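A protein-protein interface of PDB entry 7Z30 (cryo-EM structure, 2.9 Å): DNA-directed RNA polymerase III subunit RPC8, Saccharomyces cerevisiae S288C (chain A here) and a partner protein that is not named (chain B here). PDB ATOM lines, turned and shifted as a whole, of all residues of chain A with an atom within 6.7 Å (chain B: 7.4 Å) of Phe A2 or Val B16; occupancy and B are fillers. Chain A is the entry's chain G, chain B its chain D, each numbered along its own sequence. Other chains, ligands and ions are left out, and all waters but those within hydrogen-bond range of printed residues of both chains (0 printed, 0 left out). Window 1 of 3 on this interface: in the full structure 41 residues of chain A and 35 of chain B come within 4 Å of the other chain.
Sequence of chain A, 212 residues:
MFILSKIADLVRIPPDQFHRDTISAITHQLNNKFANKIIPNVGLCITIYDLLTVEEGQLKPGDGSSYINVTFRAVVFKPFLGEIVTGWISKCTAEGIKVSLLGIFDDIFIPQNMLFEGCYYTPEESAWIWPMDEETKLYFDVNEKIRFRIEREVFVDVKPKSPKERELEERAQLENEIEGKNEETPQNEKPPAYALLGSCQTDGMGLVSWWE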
ATOM      1  N   PHE A   2      -0.784 -20.304  -1.282  1.00  0.00           N
ATOM      2  CA  PHE A   2      -0.395 -21.030  -2.486  1.00  0.00           C
ATOM      3  C   PHE A   2      -1.389 -20.824  -3.623  1.00  0.00           C
ATOM      4  O   PHE A   2      -2.525 -21.293  -3.566  1.00  0.00           O
ATOM      5  CB  PHE A   2      -0.237 -22.521  -2.187  1.00  0.00           C
ATOM      6  CG  PHE A   2       1.065 -22.877  -1.524  1.00  0.00           C
ATOM      7  CD1 PHE A   2       1.855 -21.908  -0.935  1.00  0.00           C
ATOM      8  CD2 PHE A   2       1.512 -24.185  -1.519  1.00  0.00           C
ATOM      9  CE1 PHE A   2       3.056 -22.243  -0.338  1.00  0.00           C
ATOM     10  CE2 PHE A   2       2.708 -24.522  -0.919  1.00  0.00           C
ATOM     11  CZ  PHE A   2       3.481 -23.550  -0.329  1.00  0.00           C
ATOM     12  N   ILE A   3      -0.945 -20.112  -4.656  1.00  0.00           N
ATOM     13  CA  ILE A   3      -1.747 -19.836  -5.841  1.00  0.00           C
ATOM     14  C   ILE A   3      -0.838 -19.936  -7.058  1.00  0.00           C
ATOM     15  O   ILE A   3       0.371 -19.701  -6.960  1.00  0.00           O
ATOM     16  CB  ILE A   3      -2.421 -18.448  -5.761  1.00  0.00           C
ATOM     17  CG1 ILE A   3      -3.433 -18.262  -6.893  1.00  0.00           C
ATOM     18  CG2 ILE A   3      -1.377 -17.345  -5.809  1.00  0.00           C
ATOM     19  CD1 ILE A   3      -4.207 -16.968  -6.811  1.00  0.00           C
ATOM     20  N   LEU A   4      -1.412 -20.308  -8.198  1.00  0.00           N
ATOM     21  CA  LEU A   4      -0.646 -20.348  -9.431  1.00  0.00           C
ATOM     22  C   LEU A   4      -0.494 -18.942 -10.010  1.00  0.00           C
ATOM     23  O   LEU A   4      -1.017 -17.958  -9.479  1.00  0.00           O
ATOM     24  CB  LEU A   4      -1.315 -21.266 -10.450  1.00  0.00           C
ATOM     25  CG  LEU A   4      -0.913 -22.740 -10.402  1.00  0.00           C
ATOM     26  CD1 LEU A   4      -1.358 -23.442 -11.654  1.00  0.00           C
ATOM     27  CD2 LEU A   4       0.577 -22.904 -10.206  1.00  0.00           C
ATOM     28  N   ILE A  46       7.924 -21.074  -5.788  1.00  0.00           N
ATOM     29  CA  ILE A  46       8.559 -22.298  -5.312  1.00  0.00           C
ATOM     30  C   ILE A  46       9.103 -23.115  -6.475  1.00  0.00           C
ATOM     31  O   ILE A  46      10.281 -23.476  -6.501  1.00  0.00           O
ATOM     32  CB  ILE A  46       7.565 -23.121  -4.459  1.00  0.00           C
ATOM     33  CG1 ILE A  46       7.357 -22.487  -3.078  1.00  0.00           C
ATOM     34  CG2 ILE A  46       8.055 -24.551  -4.300  1.00  0.00           C
ATOM     35  CD1 ILE A  46       6.449 -21.270  -3.064  1.00  0.00           C
ATOM     36  N   TYR A  49       4.633 -24.995 -12.421  1.00  0.00           N
ATOM     37  CA  TYR A  49       3.659 -26.078 -12.486  1.00  0.00           C
ATOM     38  C   TYR A  49       3.749 -26.819 -13.814  1.00  0.00           C
ATOM     39  O   TYR A  49       4.039 -28.020 -13.853  1.00  0.00           O
ATOM     40  CB  TYR A  49       2.250 -25.519 -12.276  1.00  0.00           C
ATOM     41  CG  TYR A  49       1.280 -26.484 -11.641  1.00  0.00           C
ATOM     42  CD1 TYR A  49       1.442 -26.904 -10.328  1.00  0.00           C
ATOM     43  CD2 TYR A  49       0.199 -26.976 -12.356  1.00  0.00           C
ATOM     44  CE1 TYR A  49       0.554 -27.785  -9.747  1.00  0.00           C
ATOM     45  CE2 TYR A  49      -0.695 -27.857 -11.785  1.00  0.00           C
ATOM     46  CZ  TYR A  49      -0.513 -28.258 -10.479  1.00  0.00           C
ATOM     47  OH  TYR A  49      -1.402 -29.135  -9.907  1.00  0.00           O
ATOM     48  N   VAL A  75       3.885 -21.915  -9.015  1.00  0.00           N
ATOM     49  CA  VAL A  75       3.245 -21.906  -7.703  1.00  0.00           C
ATOM     50  C   VAL A  75       3.783 -20.729  -6.894  1.00  0.00           C
ATOM     51  O   VAL A  75       5.000 -20.541  -6.779  1.00  0.00           O
ATOM     52  CB  VAL A  75       3.459 -23.242  -6.973  1.00  0.00           C
ATOM     53  CG1 VAL A  75       2.768 -24.367  -7.723  1.00  0.00           C
ATOM     54  CG2 VAL A  75       4.936 -23.560  -6.852  1.00  0.00           C
ATOM     55  N   VAL A  76       2.875 -19.920  -6.351  1.00  0.00           N
ATOM     56  CA  VAL A  76       3.220 -18.698  -5.632  1.00  0.00           C
ATOM     57  C   VAL A  76       2.544 -18.716  -4.267  1.00  0.00           C
ATOM     58  O   VAL A  76       1.368 -19.082  -4.155  1.00  0.00           O
ATOM     59  CB  VAL A  76       2.814 -17.438  -6.418  1.00  0.00           C
ATOM     60  CG1 VAL A  76       3.548 -16.218  -5.882  1.00  0.00           C
ATOM     61  CG2 VAL A  76       3.098 -17.614  -7.905  1.00  0.00           C
ATOM     62  N   PHE A  77       3.284 -18.306  -3.237  1.00  0.00           N
ATOM     63  CA  PHE A  77       2.759 -18.167  -1.878  1.00  0.00           C
ATOM     64  C   PHE A  77       2.129 -16.784  -1.741  1.00  0.00           C
ATOM     65  O   PHE A  77       2.831 -15.783  -1.580  1.00  0.00           O
ATOM     66  CB  PHE A  77       3.873 -18.383  -0.858  1.00  0.00           C
ATOM     67  CG  PHE A  77       3.420 -18.288   0.575  1.00  0.00           C
ATOM     68  CD1 PHE A  77       2.877 -19.385   1.221  1.00  0.00           C
ATOM     69  CD2 PHE A  77       3.559 -17.105   1.282  1.00  0.00           C
ATOM     70  CE1 PHE A  77       2.462 -19.302   2.540  1.00  0.00           C
ATOM     71  CE2 PHE A  77       3.149 -17.016   2.605  1.00  0.00           C
ATOM     72  CZ  PHE A  77       2.599 -18.115   3.232  1.00  0.00           C
ATOM     73  N   LYS A  78       0.798 -16.724  -1.805  1.00  0.00           N
ATOM     74  CA  LYS A  78       0.054 -15.462  -1.790  1.00  0.00           C
ATOM     75  C   LYS A  78      -1.104 -15.479  -0.803  1.00  0.00           C
ATOM     76  O   LYS A  78      -2.254 -15.736  -1.181  1.00  0.00           O
ATOM     77  CB  LYS A  78      -0.466 -15.108  -3.185  1.00  0.00           C
ATOM     78  CG  LYS A  78       0.485 -14.272  -4.000  1.00  0.00           C
ATOM     79  CD  LYS A  78       0.546 -12.884  -3.393  1.00  0.00           C
ATOM     80  CE  LYS A  78       1.217 -11.909  -4.313  1.00  0.00           C
ATOM     81  NZ  LYS A  78       2.161 -11.084  -3.542  1.00  0.00           N
ATOM     82  N   PRO A  79      -0.844 -15.195   0.469  1.00  0.00           N
ATOM     83  CA  PRO A  79      -1.943 -14.794   1.357  1.00  0.00           C
ATOM     84  C   PRO A  79      -2.423 -13.386   1.025  1.00  0.00           C
ATOM     85  O   PRO A  79      -1.624 -12.504   0.703  1.00  0.00           O
ATOM     86  CB  PRO A  79      -1.320 -14.866   2.758  1.00  0.00           C
ATOM     87  CG  PRO A  79      -0.083 -15.680   2.601  1.00  0.00           C
ATOM     88  CD  PRO A  79       0.403 -15.451   1.213  1.00  0.00           C
ATOM     89  N   GLU A  83      -5.951 -15.752   5.628  1.00  0.00           N
ATOM     90  CA  GLU A  83      -5.137 -16.948   5.784  1.00  0.00           C
ATOM     91  C   GLU A  83      -4.499 -17.030   7.167  1.00  0.00           C
ATOM     92  O   GLU A  83      -3.912 -16.062   7.659  1.00  0.00           O
ATOM     93  CB  GLU A  83      -4.079 -17.029   4.682  1.00  0.00           C
ATOM     94  CG  GLU A  83      -4.693 -17.130   3.287  1.00  0.00           C
ATOM     95  CD  GLU A  83      -4.770 -15.804   2.571  1.00  0.00           C
ATOM     96  OE1 GLU A  83      -4.793 -15.794   1.322  1.00  0.00           O
ATOM     97  OE2 GLU A  83      -4.776 -14.764   3.263  1.00  0.00           O
ATOM     98  N   ILE A 104      11.298 -21.577   4.357  1.00  0.00           N
ATOM     99  CA  ILE A 104      10.723 -21.136   3.091  1.00  0.00           C
ATOM    100  C   ILE A 104      10.985 -19.649   2.891  1.00  0.00           C
ATOM    101  O   ILE A 104      11.484 -19.220   1.845  1.00  0.00           O
ATOM    102  CB  ILE A 104       9.217 -21.445   3.047  1.00  0.00           C
ATOM    103  CG1 ILE A 104       8.966 -22.925   3.334  1.00  0.00           C
ATOM    104  CG2 ILE A 104       8.629 -21.056   1.699  1.00  0.00           C
ATOM    105  CD1 ILE A 104       7.505 -23.298   3.359  1.00  0.00           C
ATOM    106  N   ALA B   9      -5.576 -19.771 -11.066  1.00  0.00           N
ATOM    107  CA  ALA B   9      -6.413 -20.717 -10.340  1.00  0.00           C
ATOM    108  C   ALA B   9      -5.836 -21.007  -8.958  1.00  0.00           C
ATOM    109  O   ALA B   9      -4.618 -21.083  -8.777  1.00  0.00           O
ATOM    110  CB  ALA B   9      -6.555 -22.016 -11.136  1.00  0.00           C
ATOM    111  N   PHE B  10      -6.726 -21.157  -7.980  1.00  0.00           N
ATOM    112  CA  PHE B  10      -6.321 -21.435  -6.612  1.00  0.00           C
ATOM    113  C   PHE B  10      -5.745 -22.844  -6.490  1.00  0.00           C
ATOM    114  O   PHE B  10      -5.924 -23.702  -7.358  1.00  0.00           O
ATOM    115  CB  PHE B  10      -7.503 -21.269  -5.659  1.00  0.00           C
ATOM    116  CG  PHE B  10      -7.851 -19.842  -5.374  1.00  0.00           C
ATOM    117  CD1 PHE B  10      -7.167 -19.137  -4.399  1.00  0.00           C
ATOM    118  CD2 PHE B  10      -8.850 -19.199  -6.085  1.00  0.00           C
ATOM    119  CE1 PHE B  10      -7.478 -17.822  -4.128  1.00  0.00           C
ATOM    120  CE2 PHE B  10      -9.164 -17.881  -5.820  1.00  0.00           C
ATOM    121  CZ  PHE B  10      -8.474 -17.193  -4.840  1.00  0.00           C
ATOM    122  N   LEU B  11      -5.042 -23.073  -5.383  1.00  0.00           N
ATOM    123  CA  LEU B  11      -4.407 -24.352  -5.099  1.00  0.00           C
ATOM    124  C   LEU B  11      -4.925 -24.901  -3.780  1.00  0.00           C
ATOM    125  O   LEU B  11      -4.728 -24.285  -2.727  1.00  0.00           O
ATOM    126  CB  LEU B  11      -2.883 -24.214  -5.037  1.00  0.00           C
ATOM    127  CG  LEU B  11      -2.093 -24.460  -6.321  1.00  0.00           C
ATOM    128  CD1 LEU B  11      -2.307 -25.877  -6.832  1.00  0.00           C
ATOM    129  CD2 LEU B  11      -2.491 -23.447  -7.372  1.00  0.00           C
ATOM    130  N   SER B  12      -5.575 -26.057  -3.838  1.00  0.00           N
ATOM    131  CA  SER B  12      -5.884 -26.804  -2.631  1.00  0.00           C
ATOM    132  C   SER B  12      -4.596 -27.380  -2.063  1.00  0.00           C
ATOM    133  O   SER B  12      -3.697 -27.778  -2.810  1.00  0.00           O
ATOM    134  CB  SER B  12      -6.878 -27.926  -2.929  1.00  0.00           C
ATOM    135  OG  SER B  12      -6.219 -29.053  -3.479  1.00  0.00           O
ATOM    136  N   ASP B  13      -4.497 -27.420  -0.736  1.00  0.00           N
ATOM    137  CA  ASP B  13      -3.258 -27.898  -0.138  1.00  0.00           C
ATOM    138  C   ASP B  13      -3.260 -29.417  -0.028  1.00  0.00           C
ATOM    139  O   ASP B  13      -2.936 -29.982   1.021  1.00  0.00           O
ATOM    140  CB  ASP B  13      -3.039 -27.242   1.225  1.00  0.00           C
ATOM    141  CG  ASP B  13      -2.632 -25.785   1.105  1.00  0.00           C
ATOM    142  OD1 ASP B  13      -2.141 -25.394   0.025  1.00  0.00           O
ATOM    143  OD2 ASP B  13      -2.809 -25.028   2.081  1.00  0.00           O
ATOM    144  N   TYR B  14      -3.627 -30.075  -1.125  1.00  0.00           N
ATOM    145  CA  TYR B  14      -3.312 -31.474  -1.376  1.00  0.00           C
ATOM    146  C   TYR B  14      -2.740 -31.562  -2.782  1.00  0.00           C
ATOM    147  O   TYR B  14      -1.871 -32.393  -3.064  1.00  0.00           O
ATOM    148  CB  TYR B  14      -4.545 -32.367  -1.237  1.00  0.00           C
ATOM    149  CG  TYR B  14      -4.333 -33.752  -1.807  1.00  0.00           C
ATOM    150  CD1 TYR B  14      -3.292 -34.556  -1.361  1.00  0.00           C
ATOM    151  CD2 TYR B  14      -5.159 -34.245  -2.809  1.00  0.00           C
ATOM    152  CE1 TYR B  14      -3.087 -35.817  -1.887  1.00  0.00           C
ATOM    153  CE2 TYR B  14      -4.961 -35.506  -3.340  1.00  0.00           C
ATOM    154  CZ  TYR B  14      -3.924 -36.287  -2.875  1.00  0.00           C
ATOM    155  OH  TYR B  14      -3.724 -37.542  -3.402  1.00  0.00           O
ATOM    156  N   GLU B  15      -3.225 -30.685  -3.665  1.00  0.00           N
ATOM    157  CA  GLU B  15      -2.683 -30.614  -5.016  1.00  0.00           C
ATOM    158  C   GLU B  15      -1.212 -30.231  -4.982  1.00  0.00           C
ATOM    159  O   GLU B  15      -0.395 -30.802  -5.711  1.00  0.00           O
ATOM    160  CB  GLU B  15      -3.482 -29.610  -5.849  1.00  0.00           C
ATOM    161  CG  GLU B  15      -4.706 -30.204  -6.529  1.00  0.00           C
ATOM    162  CD  GLU B  15      -5.305 -29.279  -7.573  1.00  0.00           C
ATOM    163  OE1 GLU B  15      -4.616 -28.326  -7.995  1.00  0.00           O
ATOM    164  OE2 GLU B  15      -6.470 -29.503  -7.966  1.00  0.00           O
ATOM    165  N   VAL B  16      -0.854 -29.280  -4.120  1.00  0.00           N
ATOM    166  CA  VAL B  16       0.543 -28.896  -3.966  1.00  0.00           C
ATOM    167  C   VAL B  16       1.362 -30.057  -3.416  1.00  0.00           C
ATOM    168  O   VAL B  16       2.488 -30.305  -3.864  1.00  0.00           O
ATOM    169  CB  VAL B  16       0.653 -27.650  -3.070  1.00  0.00           C
ATOM    170  CG1 VAL B  16       2.099 -27.408  -2.684  1.00  0.00           C
ATOM    171  CG2 VAL B  16       0.060 -26.438  -3.775  1.00  0.00           C
ATOM    172  N   LEU B  17       0.823 -30.775  -2.426  1.00  0.00           N
ATOM    173  CA  LEU B  17       1.553 -31.903  -1.855  1.00  0.00           C
ATOM    174  C   LEU B  17       1.830 -32.968  -2.906  1.00  0.00           C
ATOM    175  O   LEU B  17       2.958 -33.459  -3.025  1.00  0.00           O
ATOM    176  CB  LEU B  17       0.783 -32.513  -0.686  1.00  0.00           C
ATOM    177  CG  LEU B  17       1.519 -33.743  -0.140  1.00  0.00           C
ATOM    178  CD1 LEU B  17       2.882 -33.353   0.416  1.00  0.00           C
ATOM    179  CD2 LEU B  17       0.708 -34.504   0.889  1.00  0.00           C
ATOM    180  N   LYS B  18       0.808 -33.348  -3.677  1.00  0.00           N
ATOM    181  CA  LYS B  18       1.023 -34.369  -4.695  1.00  0.00           C
ATOM    182  C   LYS B  18       1.924 -33.861  -5.813  1.00  0.00           C
ATOM    183  O   LYS B  18       2.703 -34.641  -6.373  1.00  0.00           O
ATOM    184  CB  LYS B  18      -0.312 -34.869  -5.255  1.00  0.00           C
ATOM    185  CG  LYS B  18      -1.216 -33.799  -5.828  1.00  0.00           C
ATOM    186  CD  LYS B  18      -1.902 -34.278  -7.098  1.00  0.00           C
ATOM    187  CE  LYS B  18      -3.152 -33.465  -7.389  1.00  0.00           C
ATOM    188  NZ  LYS B  18      -4.128 -34.227  -8.216  1.00  0.00           N
ATOM    189  N   PHE B  19       1.857 -32.566  -6.140  1.00  0.00           N
ATOM    190  CA  PHE B  19       2.770 -32.010  -7.131  1.00  0.00           C
ATOM    191  C   PHE B  19       4.215 -32.116  -6.664  1.00  0.00           C
ATOM    192  O   PHE B  19       5.091 -32.554  -7.418  1.00  0.00           O
ATOM    193  CB  PHE B  19       2.412 -30.554  -7.429  1.00  0.00           C
ATOM    194  CG  PHE B  19       3.273 -29.925  -8.488  1.00  0.00           C
ATOM    195  CD1 PHE B  19       3.654 -30.648  -9.607  1.00  0.00           C
ATOM    196  CD2 PHE B  19       3.711 -28.619  -8.359  1.00  0.00           C
ATOM    197  CE1 PHE B  19       4.450 -30.076 -10.582  1.00  0.00           C
ATOM    198  CE2 PHE B  19       4.509 -28.041  -9.330  1.00  0.00           C
ATOM    199  CZ  PHE B  19       4.878 -28.770 -10.443  1.00  0.00           C
ATOM    200  N   LEU B  20       4.482 -31.735  -5.415  1.00  0.00           N
ATOM    201  CA  LEU B  20       5.846 -31.813  -4.905  1.00  0.00           C
ATOM    202  C   LEU B  20       6.293 -33.261  -4.754  1.00  0.00           C
ATOM    203  O   LEU B  20       7.474 -33.576  -4.938  1.00  0.00           O
ATOM    204  CB  LEU B  20       5.953 -31.065  -3.577  1.00  0.00           C
ATOM    205  CG  LEU B  20       6.456 -29.626  -3.700  1.00  0.00           C
ATOM    206  CD1 LEU B  20       5.307 -28.680  -4.014  1.00  0.00           C
ATOM    207  CD2 LEU B  20       7.177 -29.192  -2.437  1.00  0.00           C
ATOM    208  N   THR B  21       5.358 -34.165  -4.452  1.00  0.00           N
ATOM    209  CA  THR B  21       5.705 -35.576  -4.331  1.00  0.00           C
ATOM    210  C   THR B  21       6.082 -36.168  -5.685  1.00  0.00           C
ATOM    211  O   THR B  21       7.088 -36.884  -5.800  1.00  0.00           O
ATOM    212  CB  THR B  21       4.536 -36.345  -3.712  1.00  0.00           C
ATOM    213  OG1 THR B  21       4.487 -36.085  -2.304  1.00  0.00           O
ATOM    214  CG2 THR B  21       4.693 -37.841  -3.939  1.00  0.00           C
ATOM    215  N   ASP B  22       5.295 -35.877  -6.725  1.00  0.00           N
ATOM    216  CA  ASP B  22       5.646 -36.372  -8.050  1.00  0.00           C
ATOM    217  C   ASP B  22       6.909 -35.697  -8.566  1.00  0.00           C
ATOM    218  O   ASP B  22       7.675 -36.306  -9.314  1.00  0.00           O
ATOM    219  CB  ASP B  22       4.481 -36.202  -9.034  1.00  0.00           C
ATOM    220  CG  ASP B  22       4.133 -34.748  -9.314  1.00  0.00           C
ATOM    221  OD1 ASP B  22       5.003 -33.981  -9.779  1.00  0.00           O
ATOM    222  OD2 ASP B  22       2.960 -34.382  -9.099  1.00  0.00           O
ATOM    223  N   ILE B  58      13.818 -25.653  -1.515  1.00  0.00           N
ATOM    224  CA  ILE B  58      12.452 -25.142  -1.502  1.00  0.00           C
ATOM    225  C   ILE B  58      11.427 -26.256  -1.703  1.00  0.00           C
ATOM    226  O   ILE B  58      10.299 -26.157  -1.205  1.00  0.00           O
ATOM    227  CB  ILE B  58      12.284 -24.018  -2.540  1.00  0.00           C
ATOM    228  CG1 ILE B  58      11.350 -22.937  -1.991  1.00  0.00           C
ATOM    229  CG2 ILE B  58      11.777 -24.557  -3.870  1.00  0.00           C
ATOM    230  CD1 ILE B  58      11.211 -21.733  -2.883  1.00  0.00           C
ATOM    231  N   VAL B  62       8.672 -26.812   1.768  1.00  0.00           N
ATOM    232  CA  VAL B  62       7.218 -26.828   1.636  1.00  0.00           C
ATOM    233  C   VAL B  62       6.665 -28.213   1.945  1.00  0.00           C
ATOM    234  O   VAL B  62       5.684 -28.355   2.686  1.00  0.00           O
ATOM    235  CB  VAL B  62       6.808 -26.353   0.230  1.00  0.00           C
ATOM    236  CG1 VAL B  62       5.369 -26.744  -0.068  1.00  0.00           C
ATOM    237  CG2 VAL B  62       6.994 -24.851   0.101  1.00  0.00           C
ATOM    238  N   VAL B  63       7.287 -29.257   1.388  1.00  0.00           N
ATOM    239  CA  VAL B  63       6.750 -30.601   1.573  1.00  0.00           C
ATOM    240  C   VAL B  63       6.864 -31.032   3.032  1.00  0.00           C
ATOM    241  O   VAL B  63       5.976 -31.715   3.549  1.00  0.00           O
ATOM    242  CB  VAL B  63       7.429 -31.604   0.617  1.00  0.00           C
ATOM    243  CG1 VAL B  63       8.818 -31.993   1.099  1.00  0.00           C
ATOM    244  CG2 VAL B  63       6.556 -32.837   0.437  1.00  0.00           C
ATOM    245  N   TYR B  65       6.812 -28.902   5.639  1.00  0.00           N
ATOM    246  CA  TYR B  65       5.813 -28.127   6.362  1.00  0.00           C
ATOM    247  C   TYR B  65       4.422 -28.725   6.194  1.00  0.00           C
ATOM    248  O   TYR B  65       3.618 -28.698   7.132  1.00  0.00           O
ATOM    249  CB  TYR B  65       5.835 -26.670   5.895  1.00  0.00           C
ATOM    250  CG  TYR B  65       4.582 -25.898   6.232  1.00  0.00           C
ATOM    251  CD1 TYR B  65       4.318 -25.511   7.539  1.00  0.00           C
ATOM    252  CD2 TYR B  65       3.666 -25.549   5.248  1.00  0.00           C
ATOM    253  CE1 TYR B  65       3.177 -24.804   7.859  1.00  0.00           C
ATOM    254  CE2 TYR B  65       2.521 -24.841   5.559  1.00  0.00           C
ATOM    255  CZ  TYR B  65       2.281 -24.471   6.866  1.00  0.00           C
ATOM    256  OH  TYR B  65       1.143 -23.766   7.183  1.00  0.00           O
ATOM    257  N   LEU B  66       4.115 -29.265   5.012  1.00  0.00           N
ATOM    258  CA  LEU B  66       2.852 -29.985   4.854  1.00  0.00           C
ATOM    259  C   LEU B  66       2.858 -31.313   5.605  1.00  0.00           C
ATOM    260  O   LEU B  66       1.850 -31.686   6.215  1.00  0.00           O
ATOM    261  CB  LEU B  66       2.537 -30.223   3.376  1.00  0.00           C
ATOM    262  CG  LEU B  66       2.760 -29.095   2.370  1.00  0.00           C
ATOM    263  CD1 LEU B  66       3.015 -29.662   0.983  1.00  0.00           C
ATOM    264  CD2 LEU B  66       1.576 -28.146   2.356  1.00  0.00           C
ATOM    265  N   ILE B  95      -1.644 -34.851   5.570  1.00  0.00           N
ATOM    266  CA  ILE B  95      -1.940 -34.473   4.193  1.00  0.00           C
ATOM    267  C   ILE B  95      -1.628 -35.650   3.277  1.00  0.00           C
ATOM    268  O   ILE B  95      -2.044 -35.679   2.114  1.00  0.00           O
ATOM    269  CB  ILE B  95      -1.148 -33.217   3.775  1.00  0.00           C
ATOM    270  CG1 ILE B  95      -1.150 -32.171   4.891  1.00  0.00           C
ATOM    271  CG2 ILE B  95      -1.757 -32.591   2.531  1.00  0.00           C
ATOM    272  CD1 ILE B  95      -2.506 -31.543   5.145  1.00  0.00           C
ATOM    273  N   LEU B 121     -10.094 -23.326   0.902  1.00  0.00           N
ATOM    274  CA  LEU B 121      -8.719 -23.803   1.006  1.00  0.00           C
ATOM    275  C   LEU B 121      -8.169 -23.692   2.424  1.00  0.00           C
ATOM    276  O   LEU B 121      -7.109 -24.259   2.712  1.00  0.00           O
ATOM    277  CB  LEU B 121      -7.815 -23.037   0.037  1.00  0.00           C
ATOM    278  CG  LEU B 121      -7.507 -21.574   0.363  1.00  0.00           C
ATOM    279  CD1 LEU B 121      -6.068 -21.243   0.012  1.00  0.00           C
ATOM    280  CD2 LEU B 121      -8.458 -20.657  -0.385  1.00  0.00           C
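The backbone carbonyl oxygen of Ala B9 lies within hydrogen-bond range of the backbone NH of Leu A4 (3.3 Å).
The side-chain hydroxyl (OG) of Ser B12 is in hydrogen-bond range of the backbone NH (N) of Glu B15. N of Ile A46 sits at hydrogen-bond distance from O of Val A75 (3.1 Å). The backbone NH (N) of Ile A3 is in hydrogen-bond range of the backbone carbonyl oxygen (O) of Val A76 (2.6 Å).
Among the printed residues, merely in contact across the chains: Ile A46 with Ile B58 (3.2 Å), Phe A2 with Leu B11 (3.3 Å), Tyr A49 with Phe B19 (3.4 Å), Leu A4 with Leu B11 (3.4 Å), Phe A2 with Val B16 (3.4 Å), Phe A2 with Val B62 (3.6 Å), Ile A3 with Ala B9 (3.6 Å), Ile A104 with Val B62 (3.6 Å), Tyr A49 with Glu B15 (3.8 Å), Ile A3 with Leu B11 (3.9 Å) and Ile A46 with Val B62 (3.98 Å).
Of the 12 printed residues of chain A, 6 touch a printed residue of chain B. Of the 21 printed residues of chain B, 7 touch a printed residue of chain A. Printed residues of chain B that touch a printed residue of chain A: Ala B9, Leu B11, Glu B15, Val B16, Phe B19, Ile B58 and Val B62. Hydrophobic or aromatic side chains of chain B that line the printed part of chain A: Leu B11, Val B16, Phe B19, Ile B58 and Val B62.
Phe A2 touches just these residues of chain B: Leu B11 (3.3 Å), Val B16 (3.4 Å) and Val B62 (3.6 Å). Val B16 touches just one residue of chain A: Phe A2 (3.4 Å). Of the printed residues of chain B, Leu A4 touches Ala B9 and Leu B11. Of the printed residues of chain A, Glu B15 touches Tyr A49. Of the printed residues of chain A, Ile B58 touches Ile A46 (3.2 Å). The nearest printed residue of chain A that does not touch Ile B58 is Ile A104 (5.0 Å).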
